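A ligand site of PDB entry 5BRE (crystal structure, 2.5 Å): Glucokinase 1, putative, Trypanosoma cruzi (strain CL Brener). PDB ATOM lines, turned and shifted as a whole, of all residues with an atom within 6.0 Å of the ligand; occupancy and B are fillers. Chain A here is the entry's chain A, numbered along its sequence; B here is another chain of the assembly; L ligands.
CB of Pro 106 touches O5 of the ligand (3.8 Å). Gly 107 touches the ligand. Pro 108 touches the ligand (CD to C8, 3.6 Å). O of Pro 117 touches C10 of the ligand, 3.1 Å away. Phe 118 touches the ligand (C to C11, 3.8 Å). Asn 119 touches the ligand (ND2 to C13, 3.2 Å). Leu 146 touches the ligand (CD2 to O2, 3.9 Å). O of Leu 201 touches C4 of the ligand, 3.9 Å away. CA of Gly 202 touches O2 of the ligand, at 3.7 Å. Ser 224 touches the ligand. Met 348 of chain B touches the ligand. CZ of Phe 351 of chain B touches C12 of the ligand (3.4 Å). Phe 353 of chain B touches the ligand. Of the 26 residues printed, 17 come within 4 Å of the ligand. The nearest printed residue that does not touch the ligand is Gly 200 (4.03 Å).
N of Gly 116 sits at hydrogen-bond distance from O of Pro 108 (3.0 Å). The backbone NH (N) of Leu 146 lies within hydrogen-bond range of the side-chain amide oxygen (OD1) of Asn 144, 2.8 Å away. The backbone carbonyl oxygen (O) of Gly 202 is in hydrogen-bond range of the backbone NH (N) of Ala 196 (2.8 Å). The side-chain amide nitrogen (ND2) of Asn 144 sits at hydrogen-bond distance from the backbone carbonyl oxygen (O) of Gly 107 (2.8 Å). The backbone carbonyl oxygen of Val 105 sits at hydrogen-bond distance from the backbone NH of Asp 145.
An oxygen (O5) of the ligand sits at hydrogen-bond distance from the side-chain carboxylate of Asp 145, 2.5 Å away. The side-chain carboxylate of Glu 221 lies within hydrogen-bond range of an oxygen (O3) of the ligand (2.8 Å). The side-chain amide nitrogen of Asn 144 is in hydrogen-bond range of an oxygen (O3) of the ligand (3.0 Å). OE2 of Glu 250 lies within hydrogen-bond range of O4 of the ligand (3.2 Å).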
ATOM      1  N   VAL A 105      -0.343  -4.910 -32.850  1.00  0.00           N
ATOM      2  CA  VAL A 105       0.848  -4.183 -32.405  1.00  0.00           C
ATOM      3  C   VAL A 105       0.974  -4.196 -30.875  1.00  0.00           C
ATOM      4  O   VAL A 105      -0.021  -4.352 -30.161  1.00  0.00           O
ATOM      5  CB  VAL A 105       0.817  -2.717 -32.909  1.00  0.00           C
ATOM      6  CG1 VAL A 105       0.528  -2.666 -34.410  1.00  0.00           C
ATOM      7  CG2 VAL A 105      -0.202  -1.893 -32.099  1.00  0.00           C
ATOM      8  N   PRO A 106       2.207  -4.042 -30.359  1.00  0.00           N
ATOM      9  CA  PRO A 106       2.391  -4.237 -28.918  1.00  0.00           C
ATOM     10  C   PRO A 106       2.086  -2.987 -28.079  1.00  0.00           C
ATOM     11  O   PRO A 106       2.924  -2.509 -27.300  1.00  0.00           O
ATOM     12  CB  PRO A 106       3.872  -4.634 -28.810  1.00  0.00           C
ATOM     13  CG  PRO A 106       4.525  -3.962 -29.992  1.00  0.00           C
ATOM     14  CD  PRO A 106       3.489  -3.856 -31.077  1.00  0.00           C
ATOM     15  N   GLY A 107       0.863  -2.475 -28.217  1.00  0.00           N
ATOM     16  CA  GLY A 107       0.452  -1.311 -27.447  1.00  0.00           C
ATOM     17  C   GLY A 107      -1.055  -1.058 -27.433  1.00  0.00           C
ATOM     18  O   GLY A 107      -1.833  -1.798 -28.047  1.00  0.00           O
ATOM     19  N   PRO A 108      -1.464  -0.005 -26.716  1.00  0.00           N
ATOM     20  CA  PRO A 108      -2.887   0.362 -26.701  1.00  0.00           C
ATOM     21  C   PRO A 108      -3.347   0.803 -28.103  1.00  0.00           C
ATOM     22  O   PRO A 108      -2.689   1.621 -28.758  1.00  0.00           O
ATOM     23  CB  PRO A 108      -2.947   1.538 -25.718  1.00  0.00           C
ATOM     24  CG  PRO A 108      -1.712   1.401 -24.846  1.00  0.00           C
ATOM     25  CD  PRO A 108      -0.663   0.772 -25.752  1.00  0.00           C
ATOM     26  N   GLY A 116      -0.580   3.189 -30.217  1.00  0.00           N
ATOM     27  CA  GLY A 116       0.478   3.934 -29.539  1.00  0.00           C
ATOM     28  C   GLY A 116      -0.045   4.629 -28.286  1.00  0.00           C
ATOM     29  O   GLY A 116      -1.242   4.676 -28.044  1.00  0.00           O
ATOM     30  N   PRO A 117       0.866   5.178 -27.460  1.00  0.00           N
ATOM     31  CA  PRO A 117       2.336   5.145 -27.565  1.00  0.00           C
ATOM     32  C   PRO A 117       2.922   3.790 -27.157  1.00  0.00           C
ATOM     33  O   PRO A 117       2.270   3.021 -26.448  1.00  0.00           O
ATOM     34  CB  PRO A 117       2.775   6.200 -26.550  1.00  0.00           C
ATOM     35  CG  PRO A 117       1.677   6.195 -25.492  1.00  0.00           C
ATOM     36  CD  PRO A 117       0.389   5.909 -26.261  1.00  0.00           C
ATOM     37  N   PHE A 118       4.148   3.505 -27.586  1.00  0.00           N
ATOM     38  CA  PHE A 118       4.752   2.227 -27.257  1.00  0.00           C
ATOM     39  C   PHE A 118       5.918   2.355 -26.280  1.00  0.00           C
ATOM     40  O   PHE A 118       6.569   3.388 -26.203  1.00  0.00           O
ATOM     41  CB  PHE A 118       5.233   1.544 -28.523  1.00  0.00           C
ATOM     42  CG  PHE A 118       4.130   1.244 -29.483  1.00  0.00           C
ATOM     43  CD1 PHE A 118       3.402   0.066 -29.372  1.00  0.00           C
ATOM     44  CD2 PHE A 118       3.818   2.141 -30.496  1.00  0.00           C
ATOM     45  CE1 PHE A 118       2.380  -0.226 -30.270  1.00  0.00           C
ATOM     46  CE2 PHE A 118       2.801   1.858 -31.393  1.00  0.00           C
ATOM     47  CZ  PHE A 118       2.078   0.689 -31.282  1.00  0.00           C
ATOM     48  N   ASN A 119       6.151   1.285 -25.537  1.00  0.00           N
ATOM     49  CA  ASN A 119       7.280   1.245 -24.625  1.00  0.00           C
ATOM     50  C   ASN A 119       8.519   0.704 -25.328  1.00  0.00           C
ATOM     51  O   ASN A 119       9.654   1.012 -24.943  1.00  0.00           O
ATOM     52  CB  ASN A 119       6.934   0.417 -23.381  1.00  0.00           C
ATOM     53  CG  ASN A 119       7.923   0.626 -22.242  1.00  0.00           C
ATOM     54  OD1 ASN A 119       8.669  -0.276 -21.887  1.00  0.00           O
ATOM     55  ND2 ASN A 119       7.906   1.823 -21.657  1.00  0.00           N
ATOM     56  N   ASN A 120       8.291  -0.098 -26.366  1.00  0.00           N
ATOM     57  CA  ASN A 120       9.350  -0.705 -27.191  1.00  0.00           C
ATOM     58  C   ASN A 120       9.732   0.168 -28.382  1.00  0.00           C
ATOM     59  O   ASN A 120      10.884   0.183 -28.801  1.00  0.00           O
ATOM     60  CB  ASN A 120       8.880  -2.052 -27.772  1.00  0.00           C
ATOM     61  CG  ASN A 120       8.533  -3.070 -26.704  1.00  0.00           C
ATOM     62  OD1 ASN A 120       7.346  -3.367 -26.482  1.00  0.00           O
ATOM     63  ND2 ASN A 120       9.545  -3.659 -26.069  1.00  0.00           N
ATOM     64  N   ASN A 144      -4.685  -4.624 -30.600  1.00  0.00           N
ATOM     65  CA  ASN A 144      -3.617  -4.762 -29.610  1.00  0.00           C
ATOM     66  C   ASN A 144      -3.161  -6.238 -29.638  1.00  0.00           C
ATOM     67  O   ASN A 144      -3.972  -7.134 -29.931  1.00  0.00           O
ATOM     68  CB  ASN A 144      -4.111  -4.366 -28.216  1.00  0.00           C
ATOM     69  CG  ASN A 144      -3.244  -4.917 -27.126  1.00  0.00           C
ATOM     70  OD1 ASN A 144      -3.514  -5.998 -26.599  1.00  0.00           O
ATOM     71  ND2 ASN A 144      -2.205  -4.194 -26.749  1.00  0.00           N
ATOM     72  N   ASP A 145      -1.876  -6.508 -29.399  1.00  0.00           N
ATOM     73  CA  ASP A 145      -1.421  -7.888 -29.487  1.00  0.00           C
ATOM     74  C   ASP A 145      -2.225  -8.861 -28.630  1.00  0.00           C
ATOM     75  O   ASP A 145      -2.561  -9.938 -29.103  1.00  0.00           O
ATOM     76  CB  ASP A 145       0.106  -8.056 -29.287  1.00  0.00           C
ATOM     77  CG  ASP A 145       0.613  -7.565 -27.917  1.00  0.00           C
ATOM     78  OD1 ASP A 145      -0.192  -7.247 -27.026  1.00  0.00           O
ATOM     79  OD2 ASP A 145       1.855  -7.514 -27.716  1.00  0.00           O
ATOM     80  N   LEU A 146      -2.586  -8.477 -27.404  1.00  0.00           N
ATOM     81  CA  LEU A 146      -3.309  -9.404 -26.537  1.00  0.00           C
ATOM     82  C   LEU A 146      -4.783  -9.478 -26.890  1.00  0.00           C
ATOM     83  O   LEU A 146      -5.459 -10.452 -26.555  1.00  0.00           O
ATOM     84  CB  LEU A 146      -3.099  -9.082 -25.055  1.00  0.00           C
ATOM     85  CG  LEU A 146      -2.093 -10.023 -24.397  1.00  0.00           C
ATOM     86  CD1 LEU A 146      -2.570 -11.488 -24.477  1.00  0.00           C
ATOM     87  CD2 LEU A 146      -0.736  -9.867 -25.085  1.00  0.00           C
ATOM     88  N   ALA A 196      -0.285 -12.592 -20.735  1.00  0.00           N
ATOM     89  CA  ALA A 196       0.889 -13.003 -21.495  1.00  0.00           C
ATOM     90  C   ALA A 196       2.170 -12.451 -20.877  1.00  0.00           C
ATOM     91  O   ALA A 196       2.596 -11.346 -21.193  1.00  0.00           O
ATOM     92  CB  ALA A 196       0.758 -12.551 -22.954  1.00  0.00           C
ATOM     93  N   GLY A 200       6.999  -7.742 -22.314  1.00  0.00           N
ATOM     94  CA  GLY A 200       6.091  -7.003 -21.451  1.00  0.00           C
ATOM     95  C   GLY A 200       5.115  -7.920 -20.726  1.00  0.00           C
ATOM     96  O   GLY A 200       5.318  -9.144 -20.673  1.00  0.00           O
ATOM     97  N   LEU A 201       4.062  -7.340 -20.166  1.00  0.00           N
ATOM     98  CA  LEU A 201       2.977  -8.108 -19.566  1.00  0.00           C
ATOM     99  C   LEU A 201       1.662  -7.741 -20.236  1.00  0.00           C
ATOM    100  O   LEU A 201       1.146  -6.642 -20.073  1.00  0.00           O
ATOM    101  CB  LEU A 201       2.907  -7.870 -18.042  1.00  0.00           C
ATOM    102  CG  LEU A 201       1.782  -8.583 -17.307  1.00  0.00           C
ATOM    103  CD1 LEU A 201       1.890 -10.119 -17.396  1.00  0.00           C
ATOM    104  CD2 LEU A 201       1.700  -8.127 -15.854  1.00  0.00           C
ATOM    105  N   GLY A 202       1.137  -8.656 -21.036  1.00  0.00           N
ATOM    106  CA  GLY A 202      -0.060  -8.399 -21.812  1.00  0.00           C
ATOM    107  C   GLY A 202      -1.269  -8.965 -21.089  1.00  0.00           C
ATOM    108  O   GLY A 202      -1.205  -9.998 -20.402  1.00  0.00           O
ATOM    109  N   SER A 203      -2.397  -8.287 -21.236  1.00  0.00           N
ATOM    110  CA  SER A 203      -3.619  -8.766 -20.647  1.00  0.00           C
ATOM    111  C   SER A 203      -4.800  -8.470 -21.583  1.00  0.00           C
ATOM    112  O   SER A 203      -4.882  -7.379 -22.171  1.00  0.00           O
ATOM    113  CB  SER A 203      -3.825  -8.088 -19.304  1.00  0.00           C
ATOM    114  OG  SER A 203      -3.891  -6.676 -19.484  1.00  0.00           O
ATOM    115  N   LEU A 220      -6.940  -5.000 -22.377  1.00  0.00           N
ATOM    116  CA  LEU A 220      -6.710  -4.448 -21.064  1.00  0.00           C
ATOM    117  C   LEU A 220      -5.257  -4.014 -20.946  1.00  0.00           C
ATOM    118  O   LEU A 220      -4.412  -4.490 -21.696  1.00  0.00           O
ATOM    119  CB  LEU A 220      -7.010  -5.512 -20.009  1.00  0.00           C
ATOM    120  CG  LEU A 220      -8.487  -5.912 -19.839  1.00  0.00           C
ATOM    121  CD1 LEU A 220      -8.645  -6.804 -18.621  1.00  0.00           C
ATOM    122  CD2 LEU A 220      -9.379  -4.701 -19.712  1.00  0.00           C
ATOM    123  N   GLU A 221      -4.975  -3.106 -20.019  1.00  0.00           N
ATOM    124  CA  GLU A 221      -3.594  -2.766 -19.674  1.00  0.00           C
ATOM    125  C   GLU A 221      -3.335  -3.038 -18.200  1.00  0.00           C
ATOM    126  O   GLU A 221      -2.920  -2.140 -17.456  1.00  0.00           O
ATOM    127  CB  GLU A 221      -3.304  -1.284 -19.964  1.00  0.00           C
ATOM    128  CG  GLU A 221      -3.264  -0.935 -21.409  1.00  0.00           C
ATOM    129  CD  GLU A 221      -2.093  -1.630 -22.153  1.00  0.00           C
ATOM    130  OE1 GLU A 221      -1.129  -2.116 -21.501  1.00  0.00           O
ATOM    131  OE2 GLU A 221      -2.139  -1.670 -23.414  1.00  0.00           O
ATOM    132  N   SER A 224       0.184  -2.168 -16.430  1.00  0.00           N
ATOM    133  CA  SER A 224       0.586  -0.810 -16.081  1.00  0.00           C
ATOM    134  C   SER A 224      -0.044  -0.276 -14.805  1.00  0.00           C
ATOM    135  O   SER A 224       0.219   0.858 -14.424  1.00  0.00           O
ATOM    136  CB  SER A 224       0.321   0.154 -17.252  1.00  0.00           C
ATOM    137  OG  SER A 224       1.109  -0.192 -18.387  1.00  0.00           O
ATOM    138  N   GLU A 250       4.010  -4.910 -14.272  1.00  0.00           N
ATOM    139  CA  GLU A 250       4.996  -5.200 -15.292  1.00  0.00           C
ATOM    140  C   GLU A 250       6.437  -4.994 -14.812  1.00  0.00           C
ATOM    141  O   GLU A 250       7.366  -5.724 -15.234  1.00  0.00           O
ATOM    142  CB  GLU A 250       4.723  -4.361 -16.547  1.00  0.00           C
ATOM    143  CG  GLU A 250       5.538  -4.827 -17.764  1.00  0.00           C
ATOM    144  CD  GLU A 250       5.030  -4.244 -19.081  1.00  0.00           C
ATOM    145  OE1 GLU A 250       5.307  -3.060 -19.385  1.00  0.00           O
ATOM    146  OE2 GLU A 250       4.367  -4.987 -19.839  1.00  0.00           O
ATOM    147  N   MET B 309      -5.966   3.593 -16.621  1.00  0.00           N
ATOM    148  CA  MET B 309      -4.915   2.814 -17.221  1.00  0.00           C
ATOM    149  C   MET B 309      -5.376   1.409 -17.587  1.00  0.00           C
ATOM    150  O   MET B 309      -5.131   0.943 -18.719  1.00  0.00           O
ATOM    151  CB  MET B 309      -3.713   2.710 -16.267  1.00  0.00           C
ATOM    152  CG  MET B 309      -2.520   2.122 -16.938  1.00  0.00           C
ATOM    153  SD  MET B 309      -1.970   3.255 -18.228  1.00  0.00           S
ATOM    154  CE  MET B 309      -1.877   2.229 -19.716  1.00  0.00           C
ATOM    155  N   MET B 348       1.801   6.555 -14.963  1.00  0.00           N
ATOM    156  CA  MET B 348       1.547   6.401 -16.393  1.00  0.00           C
ATOM    157  C   MET B 348       1.109   7.719 -17.028  1.00  0.00           C
ATOM    158  O   MET B 348       1.077   7.839 -18.266  1.00  0.00           O
ATOM    159  CB  MET B 348       0.571   5.250 -16.664  1.00  0.00           C
ATOM    160  CG  MET B 348       1.150   3.903 -16.306  1.00  0.00           C
ATOM    161  SD  MET B 348       2.648   3.528 -17.255  1.00  0.00           S
ATOM    162  CE  MET B 348       1.925   3.242 -18.884  1.00  0.00           C
ATOM    163  N   ARG B 350       2.759  10.283 -17.298  1.00  0.00           N
ATOM    164  CA  ARG B 350       3.882  10.830 -18.070  1.00  0.00           C
ATOM    165  C   ARG B 350       3.730  10.559 -19.563  1.00  0.00           C
ATOM    166  O   ARG B 350       4.441  11.136 -20.385  1.00  0.00           O
ATOM    167  CB  ARG B 350       5.252  10.342 -17.527  1.00  0.00           C
ATOM    168  CG  ARG B 350       5.586   8.885 -17.833  1.00  0.00           C
ATOM    169  CD  ARG B 350       6.636   8.305 -16.865  1.00  0.00           C
ATOM    170  NE  ARG B 350       7.272   7.094 -17.411  1.00  0.00           N
ATOM    171  CZ  ARG B 350       7.034   5.846 -17.001  1.00  0.00           C
ATOM    172  NH1 ARG B 350       6.179   5.583 -16.031  1.00  0.00           N
ATOM    173  NH2 ARG B 350       7.667   4.833 -17.577  1.00  0.00           N
ATOM    174  N   PHE B 351       2.779   9.696 -19.914  1.00  0.00           N
ATOM    175  CA  PHE B 351       2.445   9.399 -21.306  1.00  0.00           C
ATOM    176  C   PHE B 351       1.016   9.868 -21.650  1.00  0.00           C
ATOM    177  O   PHE B 351       0.485   9.544 -22.698  1.00  0.00           O
ATOM    178  CB  PHE B 351       2.534   7.898 -21.567  1.00  0.00           C
ATOM    179  CG  PHE B 351       3.865   7.290 -21.242  1.00  0.00           C
ATOM    180  CD1 PHE B 351       4.988   7.577 -22.017  1.00  0.00           C
ATOM    181  CD2 PHE B 351       4.011   6.420 -20.171  1.00  0.00           C
ATOM    182  CE1 PHE B 351       6.236   7.015 -21.720  1.00  0.00           C
ATOM    183  CE2 PHE B 351       5.255   5.849 -19.875  1.00  0.00           C
ATOM    184  CZ  PHE B 351       6.370   6.153 -20.663  1.00  0.00           C
ATOM    185  N   PHE B 353      -1.884   9.011 -20.436  1.00  0.00           N
ATOM    186  CA  PHE B 353      -2.988   8.090 -20.198  1.00  0.00           C
ATOM    187  C   PHE B 353      -4.133   8.601 -19.316  1.00  0.00           C
ATOM    188  O   PHE B 353      -5.300   8.490 -19.687  1.00  0.00           O
ATOM    189  CB  PHE B 353      -2.482   6.726 -19.718  1.00  0.00           C
ATOM    190  CG  PHE B 353      -1.835   5.952 -20.805  1.00  0.00           C
ATOM    191  CD1 PHE B 353      -2.586   5.487 -21.890  1.00  0.00           C
ATOM    192  CD2 PHE B 353      -0.470   5.715 -20.792  1.00  0.00           C
ATOM    193  CE1 PHE B 353      -1.974   4.771 -22.906  1.00  0.00           C
ATOM    194  CE2 PHE B 353       0.141   5.001 -21.823  1.00  0.00           C
ATOM    195  CZ  PHE B 353      -0.609   4.533 -22.879  1.00  0.00           C
HETATM  196  C1  LIG L   1       0.630  -3.992 -23.931  1.00  0.00           C
HETATM  197  C2  LIG L   1       1.924  -3.226 -23.656  1.00  0.00           C
HETATM  198  C3  LIG L   1       2.883  -4.097 -22.834  1.00  0.00           C
HETATM  199  O1  LIG L   1       3.192  -5.239 -23.628  1.00  0.00           O
HETATM  200  C4  LIG L   1       2.018  -6.072 -23.864  1.00  0.00           C
HETATM  201  C5  LIG L   1       0.919  -5.281 -24.597  1.00  0.00           C
HETATM  202  N1  LIG L   1       1.567  -2.033 -22.891  1.00  0.00           N
HETATM  203  O2  LIG L   1      -0.313  -6.055 -24.633  1.00  0.00           O
HETATM  204  O3  LIG L   1      -0.216  -3.180 -24.747  1.00  0.00           O
HETATM  205  C6  LIG L   1       2.471  -7.290 -24.662  1.00  0.00           C
HETATM  206  O4  LIG L   1       4.057  -3.436 -22.580  1.00  0.00           O
HETATM  207  O5  LIG L   1       3.302  -6.820 -25.789  1.00  0.00           O
HETATM  208  C7  LIG L   1       2.074  -0.818 -23.127  1.00  0.00           C
HETATM  209  O6  LIG L   1       1.503   0.104 -22.255  1.00  0.00           O
HETATM  210  O7  LIG L   1       2.775  -0.532 -24.070  1.00  0.00           O
HETATM  211  C8  LIG L   1       1.373   1.436 -22.833  1.00  0.00           C
HETATM  212  C9  LIG L   1       2.687   2.131 -22.650  1.00  0.00           C
HETATM  213  C10 LIG L   1       3.023   3.256 -23.445  1.00  0.00           C
HETATM  214  C11 LIG L   1       4.249   3.871 -23.240  1.00  0.00           C
HETATM  215  C12 LIG L   1       5.118   3.388 -22.278  1.00  0.00           C
HETATM  216  C13 LIG L   1       4.783   2.297 -21.495  1.00  0.00           C
HETATM  217  C14 LIG L   1       3.571   1.661 -21.681  1.00  0.00           C
